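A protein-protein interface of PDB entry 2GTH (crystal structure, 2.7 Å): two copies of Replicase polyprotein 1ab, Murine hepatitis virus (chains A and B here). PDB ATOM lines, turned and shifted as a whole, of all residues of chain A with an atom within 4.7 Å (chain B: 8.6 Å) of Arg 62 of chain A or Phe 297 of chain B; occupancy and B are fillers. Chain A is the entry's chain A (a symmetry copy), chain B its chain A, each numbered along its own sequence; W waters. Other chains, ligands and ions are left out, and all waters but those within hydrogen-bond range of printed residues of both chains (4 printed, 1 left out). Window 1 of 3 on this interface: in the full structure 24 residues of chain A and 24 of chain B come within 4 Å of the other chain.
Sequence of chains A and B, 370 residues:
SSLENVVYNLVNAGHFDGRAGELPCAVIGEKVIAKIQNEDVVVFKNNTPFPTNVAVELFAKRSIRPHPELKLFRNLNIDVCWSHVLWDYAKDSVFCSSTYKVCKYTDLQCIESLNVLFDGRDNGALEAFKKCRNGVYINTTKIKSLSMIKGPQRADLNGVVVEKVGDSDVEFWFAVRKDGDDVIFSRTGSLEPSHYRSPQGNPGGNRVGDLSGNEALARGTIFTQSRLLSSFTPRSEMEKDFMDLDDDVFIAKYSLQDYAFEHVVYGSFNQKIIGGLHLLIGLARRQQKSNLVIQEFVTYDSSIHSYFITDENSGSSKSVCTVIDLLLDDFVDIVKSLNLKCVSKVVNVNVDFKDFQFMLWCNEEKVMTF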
ATOM      1  N   LEU A  10     -13.405  19.603   9.376  1.00  0.00           N
ATOM      2  CA  LEU A  10     -13.704  20.686  10.294  1.00  0.00           C
ATOM      3  C   LEU A  10     -12.521  21.653  10.353  1.00  0.00           C
ATOM      4  O   LEU A  10     -12.680  22.873  10.271  1.00  0.00           O
ATOM      5  CB  LEU A  10     -13.973  20.146  11.698  1.00  0.00           C
ATOM      6  CG  LEU A  10     -14.617  21.210  12.590  1.00  0.00           C
ATOM      7  CD1 LEU A  10     -15.893  21.686  11.899  1.00  0.00           C
ATOM      8  CD2 LEU A  10     -14.926  20.659  13.962  1.00  0.00           C
ATOM      9  N   GLY A  14     -13.559  23.756   7.254  1.00  0.00           N
ATOM     10  CA  GLY A  14     -14.441  24.589   8.031  1.00  0.00           C
ATOM     11  C   GLY A  14     -15.780  23.927   8.225  1.00  0.00           C
ATOM     12  O   GLY A  14     -16.661  24.475   8.875  1.00  0.00           O
ATOM     13  N   HIS A  15     -15.935  22.742   7.650  1.00  0.00           N
ATOM     14  CA  HIS A  15     -17.168  21.956   7.769  1.00  0.00           C
ATOM     15  C   HIS A  15     -16.931  20.715   6.923  1.00  0.00           C
ATOM     16  O   HIS A  15     -15.810  20.498   6.471  1.00  0.00           O
ATOM     17  CB  HIS A  15     -18.375  22.756   7.261  1.00  0.00           C
ATOM     18  CG  HIS A  15     -18.348  23.011   5.788  1.00  0.00           C
ATOM     19  ND1 HIS A  15     -19.153  22.327   4.902  1.00  0.00           N
ATOM     20  CD2 HIS A  15     -17.545  23.800   5.039  1.00  0.00           C
ATOM     21  CE1 HIS A  15     -18.842  22.683   3.669  1.00  0.00           C
ATOM     22  NE2 HIS A  15     -17.869  23.573   3.724  1.00  0.00           N
ATOM     23  N   VAL A  42      -8.410  21.286  21.522  1.00  0.00           N
ATOM     24  CA  VAL A  42      -9.821  20.965  21.560  1.00  0.00           C
ATOM     25  C   VAL A  42     -10.460  21.719  20.414  1.00  0.00           C
ATOM     26  O   VAL A  42     -10.361  22.943  20.342  1.00  0.00           O
ATOM     27  CB  VAL A  42     -10.468  21.405  22.898  1.00  0.00           C
ATOM     28  CG1 VAL A  42     -11.974  21.421  22.770  1.00  0.00           C
ATOM     29  CG2 VAL A  42     -10.058  20.459  24.016  1.00  0.00           C
ATOM     30  N   VAL A  43     -11.111  20.987  19.519  1.00  0.00           N
ATOM     31  CA  VAL A  43     -11.753  21.588  18.355  1.00  0.00           C
ATOM     32  C   VAL A  43     -13.282  21.584  18.468  1.00  0.00           C
ATOM     33  O   VAL A  43     -13.961  22.280  17.720  1.00  0.00           O
ATOM     34  CB  VAL A  43     -11.358  20.840  17.055  1.00  0.00           C
ATOM     35  CG1 VAL A  43      -9.855  20.894  16.841  1.00  0.00           C
ATOM     36  CG2 VAL A  43     -11.819  19.415  17.117  1.00  0.00           C
ATOM     37  N   LEU A  58     -22.049  15.634  13.233  1.00  0.00           N
ATOM     38  CA  LEU A  58     -23.261  16.354  12.882  1.00  0.00           C
ATOM     39  C   LEU A  58     -22.869  17.806  12.706  1.00  0.00           C
ATOM     40  O   LEU A  58     -23.096  18.389  11.645  1.00  0.00           O
ATOM     41  CB  LEU A  58     -24.328  16.192  13.974  1.00  0.00           C
ATOM     42  CG  LEU A  58     -24.911  14.764  14.086  1.00  0.00           C
ATOM     43  CD1 LEU A  58     -25.822  14.638  15.304  1.00  0.00           C
ATOM     44  CD2 LEU A  58     -25.669  14.416  12.799  1.00  0.00           C
ATOM     45  N   PHE A  59     -22.239  18.373  13.725  1.00  0.00           N
ATOM     46  CA  PHE A  59     -21.800  19.769  13.667  1.00  0.00           C
ATOM     47  C   PHE A  59     -20.933  20.068  12.417  1.00  0.00           C
ATOM     48  O   PHE A  59     -21.065  21.113  11.748  1.00  0.00           O
ATOM     49  CB  PHE A  59     -21.004  20.132  14.935  1.00  0.00           C
ATOM     50  CG  PHE A  59     -20.550  21.558  14.962  1.00  0.00           C
ATOM     51  CD1 PHE A  59     -21.447  22.573  15.249  1.00  0.00           C
ATOM     52  CD2 PHE A  59     -19.246  21.888  14.575  1.00  0.00           C
ATOM     53  CE1 PHE A  59     -21.062  23.901  15.139  1.00  0.00           C
ATOM     54  CE2 PHE A  59     -18.837  23.208  14.462  1.00  0.00           C
ATOM     55  CZ  PHE A  59     -19.738  24.218  14.738  1.00  0.00           C
ATOM     56  N   ALA A  60     -20.032  19.142  12.112  1.00  0.00           N
ATOM     57  CA  ALA A  60     -19.159  19.294  10.959  1.00  0.00           C
ATOM     58  C   ALA A  60     -19.968  19.314   9.663  1.00  0.00           C
ATOM     59  O   ALA A  60     -19.560  19.948   8.691  1.00  0.00           O
ATOM     60  CB  ALA A  60     -18.140  18.167  10.933  1.00  0.00           C
ATOM     61  N   LYS A  61     -21.111  18.635   9.650  1.00  0.00           N
ATOM     62  CA  LYS A  61     -21.954  18.589   8.459  1.00  0.00           C
ATOM     63  C   LYS A  61     -23.178  19.491   8.540  1.00  0.00           C
ATOM     64  O   LYS A  61     -24.194  19.227   7.914  1.00  0.00           O
ATOM     65  CB  LYS A  61     -22.403  17.155   8.202  1.00  0.00           C
ATOM     66  CG  LYS A  61     -21.279  16.187   7.983  1.00  0.00           C
ATOM     67  CD  LYS A  61     -21.802  14.775   7.875  1.00  0.00           C
ATOM     68  CE  LYS A  61     -20.664  13.790   7.734  1.00  0.00           C
ATOM     69  NZ  LYS A  61     -21.117  12.374   7.663  1.00  0.00           N
ATOM     70  N   ARG A  62     -23.080  20.554   9.317  1.00  0.00           N
ATOM     71  CA  ARG A  62     -24.183  21.503   9.490  1.00  0.00           C
ATOM     72  C   ARG A  62     -24.351  22.375   8.226  1.00  0.00           C
ATOM     73  O   ARG A  62     -23.396  22.571   7.463  1.00  0.00           O
ATOM     74  CB  ARG A  62     -23.865  22.425  10.676  1.00  0.00           C
ATOM     75  CG  ARG A  62     -22.609  23.239  10.389  1.00  0.00           C
ATOM     76  CD  ARG A  62     -22.286  24.286  11.407  1.00  0.00           C
ATOM     77  NE  ARG A  62     -21.131  25.076  10.979  1.00  0.00           N
ATOM     78  CZ  ARG A  62     -19.899  24.597  10.815  1.00  0.00           C
ATOM     79  NH1 ARG A  62     -19.647  23.315  11.044  1.00  0.00           N
ATOM     80  NH2 ARG A  62     -18.917  25.399  10.419  1.00  0.00           N
ATOM     81  N   SER A  63     -25.553  22.910   8.020  1.00  0.00           N
ATOM     82  CA  SER A  63     -25.804  23.789   6.883  1.00  0.00           C
ATOM     83  C   SER A  63     -24.976  25.059   7.013  1.00  0.00           C
ATOM     84  O   SER A  63     -25.139  25.819   7.969  1.00  0.00           O
ATOM     85  CB  SER A  63     -27.273  24.225   6.815  1.00  0.00           C
ATOM     86  OG  SER A  63     -28.155  23.137   6.747  1.00  0.00           O
ATOM     87  N   ILE A  64     -24.096  25.302   6.056  1.00  0.00           N
ATOM     88  CA  ILE A  64     -23.308  26.513   6.093  1.00  0.00           C
ATOM     89  C   ILE A  64     -23.953  27.529   5.165  1.00  0.00           C
ATOM     90  O   ILE A  64     -23.406  28.607   4.976  1.00  0.00           O
ATOM     91  CB  ILE A  64     -21.821  26.278   5.658  1.00  0.00           C
ATOM     92  CG1 ILE A  64     -21.740  25.661   4.279  1.00  0.00           C
ATOM     93  CG2 ILE A  64     -21.130  25.345   6.613  1.00  0.00           C
ATOM     94  CD1 ILE A  64     -20.384  25.692   3.747  1.00  0.00           C
ATOM     95  N   VAL A  85     -28.591  18.671   7.702  1.00  0.00           N
ATOM     96  CA  VAL A  85     -28.800  18.832   9.126  1.00  0.00           C
ATOM     97  C   VAL A  85     -28.639  20.290   9.539  1.00  0.00           C
ATOM     98  O   VAL A  85     -27.725  20.996   9.088  1.00  0.00           O
ATOM     99  CB  VAL A  85     -27.824  17.941   9.942  1.00  0.00           C
ATOM    100  CG1 VAL A  85     -26.379  18.284   9.611  1.00  0.00           C
ATOM    101  CG2 VAL A  85     -28.042  18.159  11.415  1.00  0.00           C
ATOM    102  N   TRP A  87     -28.212  23.297  12.503  1.00  0.00           N
ATOM    103  CA  TRP A  87     -27.622  23.524  13.804  1.00  0.00           C
ATOM    104  C   TRP A  87     -28.227  24.738  14.475  1.00  0.00           C
ATOM    105  O   TRP A  87     -28.295  25.820  13.896  1.00  0.00           O
ATOM    106  CB  TRP A  87     -26.119  23.711  13.642  1.00  0.00           C
ATOM    107  CG  TRP A  87     -25.393  23.880  14.920  1.00  0.00           C
ATOM    108  CD1 TRP A  87     -25.101  25.051  15.551  1.00  0.00           C
ATOM    109  CD2 TRP A  87     -24.842  22.833  15.730  1.00  0.00           C
ATOM    110  NE1 TRP A  87     -24.395  24.801  16.707  1.00  0.00           N
ATOM    111  CE2 TRP A  87     -24.221  23.447  16.839  1.00  0.00           C
ATOM    112  CE3 TRP A  87     -24.810  21.434  15.621  1.00  0.00           C
ATOM    113  CZ2 TRP A  87     -23.574  22.711  17.834  1.00  0.00           C
ATOM    114  CZ3 TRP A  87     -24.170  20.708  16.608  1.00  0.00           C
ATOM    115  CH2 TRP A  87     -23.560  21.348  17.699  1.00  0.00           C
ATOM    116  N   TYR A  89     -27.620  27.374  16.911  1.00  0.00           N
ATOM    117  CA  TYR A  89     -26.572  28.035  17.640  1.00  0.00           C
ATOM    118  C   TYR A  89     -27.139  28.588  18.938  1.00  0.00           C
ATOM    119  O   TYR A  89     -26.397  28.925  19.853  1.00  0.00           O
ATOM    120  CB  TYR A  89     -25.972  29.128  16.768  1.00  0.00           C
ATOM    121  CG  TYR A  89     -25.159  28.597  15.614  1.00  0.00           C
ATOM    122  CD1 TYR A  89     -23.824  28.239  15.791  1.00  0.00           C
ATOM    123  CD2 TYR A  89     -25.720  28.464  14.340  1.00  0.00           C
ATOM    124  CE1 TYR A  89     -23.059  27.771  14.725  1.00  0.00           C
ATOM    125  CE2 TYR A  89     -24.971  27.994  13.257  1.00  0.00           C
ATOM    126  CZ  TYR A  89     -23.629  27.644  13.451  1.00  0.00           C
ATOM    127  OH  TYR A  89     -22.854  27.159  12.397  1.00  0.00           O
ATOM    128  N   ILE B 294     -17.070  35.835  13.930  1.00  0.00           N
ATOM    129  CA  ILE B 294     -15.965  34.949  13.626  1.00  0.00           C
ATOM    130  C   ILE B 294     -16.073  33.639  14.372  1.00  0.00           C
ATOM    131  O   ILE B 294     -16.377  33.638  15.557  1.00  0.00           O
ATOM    132  CB  ILE B 294     -14.607  35.564  14.016  1.00  0.00           C
ATOM    133  CG1 ILE B 294     -14.240  36.715  13.094  1.00  0.00           C
ATOM    134  CG2 ILE B 294     -13.537  34.506  13.933  1.00  0.00           C
ATOM    135  CD1 ILE B 294     -15.132  37.891  13.234  1.00  0.00           C
ATOM    136  N   GLN B 295     -15.843  32.537  13.663  1.00  0.00           N
ATOM    137  CA  GLN B 295     -15.825  31.200  14.262  1.00  0.00           C
ATOM    138  C   GLN B 295     -14.381  30.696  14.004  1.00  0.00           C
ATOM    139  O   GLN B 295     -13.755  31.019  12.975  1.00  0.00           O
ATOM    140  CB  GLN B 295     -16.813  30.229  13.589  1.00  0.00           C
ATOM    141  CG  GLN B 295     -18.205  30.767  13.381  1.00  0.00           C
ATOM    142  CD  GLN B 295     -19.175  29.766  12.730  1.00  0.00           C
ATOM    143  OE1 GLN B 295     -19.533  28.754  13.332  1.00  0.00           O
ATOM    144  NE2 GLN B 295     -19.609  30.062  11.498  1.00  0.00           N
ATOM    145  N   GLU B 296     -13.853  29.932  14.958  1.00  0.00           N
ATOM    146  CA  GLU B 296     -12.519  29.360  14.849  1.00  0.00           C
ATOM    147  C   GLU B 296     -12.476  28.058  15.631  1.00  0.00           C
ATOM    148  O   GLU B 296     -12.500  28.069  16.860  1.00  0.00           O
ATOM    149  CB  GLU B 296     -11.453  30.328  15.384  1.00  0.00           C
ATOM    150  CG  GLU B 296     -10.081  29.682  15.476  1.00  0.00           C
ATOM    151  CD  GLU B 296      -8.930  30.652  15.485  1.00  0.00           C
ATOM    152  OE1 GLU B 296      -8.990  31.643  16.238  1.00  0.00           O
ATOM    153  OE2 GLU B 296      -7.951  30.411  14.738  1.00  0.00           O
ATOM    154  N   PHE B 297     -12.404  26.936  14.919  1.00  0.00           N
ATOM    155  CA  PHE B 297     -12.360  25.617  15.558  1.00  0.00           C
ATOM    156  C   PHE B 297     -11.016  25.250  16.174  1.00  0.00           C
ATOM    157  O   PHE B 297     -10.967  24.495  17.143  1.00  0.00           O
ATOM    158  CB  PHE B 297     -12.806  24.565  14.551  1.00  0.00           C
ATOM    159  CG  PHE B 297     -14.030  24.977  13.809  1.00  0.00           C
ATOM    160  CD1 PHE B 297     -15.167  25.355  14.506  1.00  0.00           C
ATOM    161  CD2 PHE B 297     -14.012  25.107  12.427  1.00  0.00           C
ATOM    162  CE1 PHE B 297     -16.261  25.865  13.846  1.00  0.00           C
ATOM    163  CE2 PHE B 297     -15.106  25.619  11.749  1.00  0.00           C
ATOM    164  CZ  PHE B 297     -16.231  26.000  12.460  1.00  0.00           C
ATOM    165  N   VAL B 298      -9.934  25.789  15.616  1.00  0.00           N
ATOM    166  CA  VAL B 298      -8.603  25.547  16.150  1.00  0.00           C
ATOM    167  C   VAL B 298      -8.057  26.839  16.738  1.00  0.00           C
ATOM    168  O   VAL B 298      -7.432  27.624  16.045  1.00  0.00           O
ATOM    169  CB  VAL B 298      -7.633  25.035  15.073  1.00  0.00           C
ATOM    170  CG1 VAL B 298      -6.246  24.833  15.687  1.00  0.00           C
ATOM    171  CG2 VAL B 298      -8.138  23.716  14.505  1.00  0.00           C
ATOM    172  N   THR B 299      -8.276  27.046  18.028  1.00  0.00           N
ATOM    173  CA  THR B 299      -7.822  28.267  18.670  1.00  0.00           C
ATOM    174  C   THR B 299      -6.634  28.228  19.621  1.00  0.00           C
ATOM    175  O   THR B 299      -6.634  27.529  20.635  1.00  0.00           O
ATOM    176  CB  THR B 299      -8.952  28.945  19.463  1.00  0.00           C
ATOM    177  OG1 THR B 299      -9.559  27.979  20.332  1.00  0.00           O
ATOM    178  CG2 THR B 299      -9.990  29.527  18.537  1.00  0.00           C
ATOM    179  N   TYR B 300      -5.632  29.025  19.278  1.00  0.00           N
ATOM    180  CA  TYR B 300      -4.455  29.218  20.092  1.00  0.00           C
ATOM    181  C   TYR B 300      -3.617  30.269  19.397  1.00  0.00           C
ATOM    182  O   TYR B 300      -3.860  30.591  18.239  1.00  0.00           O
ATOM    183  CB  TYR B 300      -3.685  27.912  20.334  1.00  0.00           C
ATOM    184  CG  TYR B 300      -3.256  27.146  19.124  1.00  0.00           C
ATOM    185  CD1 TYR B 300      -2.721  27.787  18.011  1.00  0.00           C
ATOM    186  CD2 TYR B 300      -3.340  25.752  19.109  1.00  0.00           C
ATOM    187  CE1 TYR B 300      -2.278  27.051  16.898  1.00  0.00           C
ATOM    188  CE2 TYR B 300      -2.903  25.000  18.008  1.00  0.00           C
ATOM    189  CZ  TYR B 300      -2.373  25.658  16.907  1.00  0.00           C
ATOM    190  OH  TYR B 300      -1.955  24.937  15.824  1.00  0.00           O
ATOM    191  N   SER B 306      -7.451  31.191  10.990  1.00  0.00           N
ATOM    192  CA  SER B 306      -8.328  30.711   9.963  1.00  0.00           C
ATOM    193  C   SER B 306      -9.705  30.755  10.591  1.00  0.00           C
ATOM    194  O   SER B 306     -10.054  29.936  11.451  1.00  0.00           O
ATOM    195  CB  SER B 306      -7.924  29.302   9.560  1.00  0.00           C
ATOM    196  OG  SER B 306      -8.786  28.802   8.565  1.00  0.00           O
ATOM    197  N   TYR B 307     -10.485  31.742  10.176  1.00  0.00           N
ATOM    198  CA  TYR B 307     -11.805  31.904  10.724  1.00  0.00           C
ATOM    199  C   TYR B 307     -12.912  31.484   9.752  1.00  0.00           C
ATOM    200  O   TYR B 307     -12.671  31.216   8.574  1.00  0.00           O
ATOM    201  CB  TYR B 307     -12.005  33.361  11.138  1.00  0.00           C
ATOM    202  CG  TYR B 307     -10.959  33.923  12.092  1.00  0.00           C
ATOM    203  CD1 TYR B 307     -10.543  33.204  13.215  1.00  0.00           C
ATOM    204  CD2 TYR B 307     -10.454  35.223  11.915  1.00  0.00           C
ATOM    205  CE1 TYR B 307      -9.660  33.764  14.149  1.00  0.00           C
ATOM    206  CE2 TYR B 307      -9.568  35.792  12.836  1.00  0.00           C
ATOM    207  CZ  TYR B 307      -9.177  35.056  13.957  1.00  0.00           C
ATOM    208  OH  TYR B 307      -8.328  35.623  14.894  1.00  0.00           O
ATOM    209  N   PHE B 308     -14.123  31.374  10.285  1.00  0.00           N
ATOM    210  CA  PHE B 308     -15.282  31.075   9.477  1.00  0.00           C
ATOM    211  C   PHE B 308     -16.055  32.392   9.620  1.00  0.00           C
ATOM    212  O   PHE B 308     -16.814  32.575  10.565  1.00  0.00           O
ATOM    213  CB  PHE B 308     -16.091  29.919  10.064  1.00  0.00           C
ATOM    214  CG  PHE B 308     -17.009  29.288   9.069  1.00  0.00           C
ATOM    215  CD1 PHE B 308     -16.772  27.995   8.607  1.00  0.00           C
ATOM    216  CD2 PHE B 308     -18.045  30.031   8.498  1.00  0.00           C
ATOM    217  CE1 PHE B 308     -17.545  27.461   7.590  1.00  0.00           C
ATOM    218  CE2 PHE B 308     -18.816  29.511   7.485  1.00  0.00           C
ATOM    219  CZ  PHE B 308     -18.573  28.226   7.023  1.00  0.00           C
ATOM    220  N   ILE B 309     -15.857  33.321   8.697  1.00  0.00           N
ATOM    221  CA  ILE B 309     -16.511  34.610   8.826  1.00  0.00           C
ATOM    222  C   ILE B 309     -17.873  34.704   8.159  1.00  0.00           C
ATOM    223  O   ILE B 309     -18.115  34.098   7.125  1.00  0.00           O
ATOM    224  CB  ILE B 309     -15.587  35.731   8.285  1.00  0.00           C
ATOM    225  CG1 ILE B 309     -14.318  35.787   9.137  1.00  0.00           C
ATOM    226  CG2 ILE B 309     -16.316  37.070   8.275  1.00  0.00           C
ATOM    227  CD1 ILE B 309     -13.201  36.597   8.540  1.00  0.00           C
ATOM    228  N   THR B 310     -18.756  35.474   8.777  1.00  0.00           N
ATOM    229  CA  THR B 310     -20.093  35.692   8.268  1.00  0.00           C
ATOM    230  C   THR B 310     -20.362  37.169   8.489  1.00  0.00           C
ATOM    231  O   THR B 310     -20.160  37.662   9.590  1.00  0.00           O
ATOM    232  CB  THR B 310     -21.118  34.869   9.058  1.00  0.00           C
ATOM    233  OG1 THR B 310     -20.715  33.504   9.036  1.00  0.00           O
ATOM    234  CG2 THR B 310     -22.502  34.970   8.439  1.00  0.00           C
ATOM    235  N   LYS B 318     -17.555  33.201   4.379  1.00  0.00           N
ATOM    236  CA  LYS B 318     -16.486  32.369   3.856  1.00  0.00           C
ATOM    237  C   LYS B 318     -16.105  31.347   4.926  1.00  0.00           C
ATOM    238  O   LYS B 318     -15.880  31.712   6.085  1.00  0.00           O
ATOM    239  CB  LYS B 318     -15.275  33.244   3.506  1.00  0.00           C
ATOM    240  CG  LYS B 318     -14.448  32.710   2.366  1.00  0.00           C
ATOM    241  CD  LYS B 318     -13.080  33.329   2.336  1.00  0.00           C
ATOM    242  CE  LYS B 318     -13.098  34.794   1.988  1.00  0.00           C
ATOM    243  NZ  LYS B 318     -11.708  35.309   1.728  1.00  0.00           N
ATOM    244  N   SER B 319     -16.043  30.076   4.525  1.00  0.00           N
ATOM    245  CA  SER B 319     -15.714  28.974   5.424  1.00  0.00           C
ATOM    246  C   SER B 319     -14.290  29.092   5.926  1.00  0.00           C
ATOM    247  O   SER B 319     -14.006  29.014   7.131  1.00  0.00           O
ATOM    248  CB  SER B 319     -15.832  27.635   4.708  1.00  0.00           C
ATOM    249  OG  SER B 319     -16.867  27.649   3.756  1.00  0.00           O
ATOM    250  N   VAL B 320     -13.380  29.247   4.976  1.00  0.00           N
ATOM    251  CA  VAL B 320     -11.983  29.372   5.313  1.00  0.00           C
ATOM    252  C   VAL B 320     -11.441  30.670   4.754  1.00  0.00           C
ATOM    253  O   VAL B 320     -11.247  30.824   3.550  1.00  0.00           O
ATOM    254  CB  VAL B 320     -11.189  28.187   4.787  1.00  0.00           C
ATOM    255  CG1 VAL B 320      -9.751  28.311   5.194  1.00  0.00           C
ATOM    256  CG2 VAL B 320     -11.779  26.907   5.333  1.00  0.00           C
HETATM  257  O   HOH W   1     -20.285  27.813  10.339  1.00  0.00           O
HETATM  258  O   HOH W   2      -9.834  25.540  19.562  1.00  0.00           O
HETATM  259  O   HOH W   3     -17.745  25.745   1.276  1.00  0.00           O
HETATM  260  O   HOH W   4     -15.236  25.162   2.741  1.00  0.00           O
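Of the printed residues of chain B, Leu 10 of chain A touches Phe 297 (3.4 Å). Of the printed residues of chain B, Gly 14 of chain A touches Phe 297 (3.5 Å) and Phe 308 (3.4 Å). Leu 58 of chain A touches none of the printed residues of chain B. Arg 62 of chain A touches just these residues of chain B: Phe 297 and Phe 308. Ser 63 of chain A touches none of the printed residues of chain B. Of the printed residues of chain B, Ile 64 of chain A touches Phe 308 (3.9 Å). Printed residues of chain A within 4 Å of Gln 295 of chain B: Tyr 89 (3.8 Å). Phe 297 of chain B touches just these residues of chain A: Leu 10 (3.4 Å), Gly 14 (3.5 Å), Val 42 (3.6 Å), Val 43 (3.2 Å), Phe 59 (3.8 Å) and Arg 62 (3.4 Å). The nearest residue of chain B that does not touch Arg 62 of chain A is Gln 295 of chain B (4.5 Å). The nearest printed residue of chain A that does not touch Phe 297 of chain B is His 15 of chain A (5.1 Å).
Water W2 lies within hydrogen-bond range of OG1 of Thr 299 of chain B (2.6 Å), O of Val 42 of chain A (2.8 Å) and O of Phe 297 of chain B (2.9 Å). Water W1 lies within hydrogen-bond range of NE2 of Gln 295 of chain B (2.6 Å), NH2 of Arg 62 of chain A (2.8 Å) and OH of Tyr 89 of chain A (3.4 Å). Water W4 lies within hydrogen-bond range of the side-chain hydroxyl of Ser 319 of chain B and a ring nitrogen (NE2) of His 15 of chain A. Water W3 bridges OG of Ser 319 of chain B (3.2 Å) and NE2 of His 15 of chain A (3.3 Å).
The backbone carbonyl oxygen (O) of Gln 295 of chain B is in hydrogen-bond range of the backbone NH (N) of Phe 308 of chain B, 2.7 Å away. O of Gly 14 of chain A sits at hydrogen-bond distance from NH2 of Arg 62 of chain A, at 2.9 Å. The guanidinium group (NH1) of Arg 62 of chain A sits at hydrogen-bond distance from the backbone carbonyl oxygen (O) of Phe 59 of chain A (2.7 Å). The side-chain hydroxyl of Tyr 89 of chain A is in hydrogen-bond range of the guanidinium group of Arg 62 of chain A (3.1 Å).
No position is printed for both chains. Of the 10 pairs that touch across the chains among the printed residues, none has its exchanged pair printed and touching as well.
O of Leu 10 of chain A touches CD2 of Phe 297 of chain B, 3.4 Å away. O of Gly 14 of chain A touches CE2 of Phe 297 of chain B (3.5 Å). Phe 308 of chain B touches Gly 14 of chain A. O of Val 42 of chain A touches O of Phe 297 of chain B, at 3.6 Å. Val 43 of chain A touches Phe 297 of chain B (CA to O, 3.2 Å). Phe 59 of chain A touches Phe 297 of chain B. Arg 62 of chain A touches Phe 297 of chain B (NH2 to CZ, 3.4 Å). NH2 of Arg 62 of chain A touches CE1 of Phe 308 of chain B, 3.8 Å away. CZ of Phe 308 of chain B touches CG2 of Ile 64 of chain A (3.9 Å). OE1 of Gln 295 of chain B touches OH of Tyr 89 of chain A, at 3.8 Å.
Of the 15 printed residues of chain B, 3 touch a printed residue of chain A. Hydrophobic or aromatic side chains of chain B that line the printed part of chain A: Phe 297 and Phe 308. Of the 15 printed residues of chain A, 8 touch a printed residue of chain B. Among the printed residues, 10 pairs touch across the chains. Among the printed residues, no Asp or Glu carboxylate lies within 4 Å of a Lys or Arg side-chain nitrogen of the other chain.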
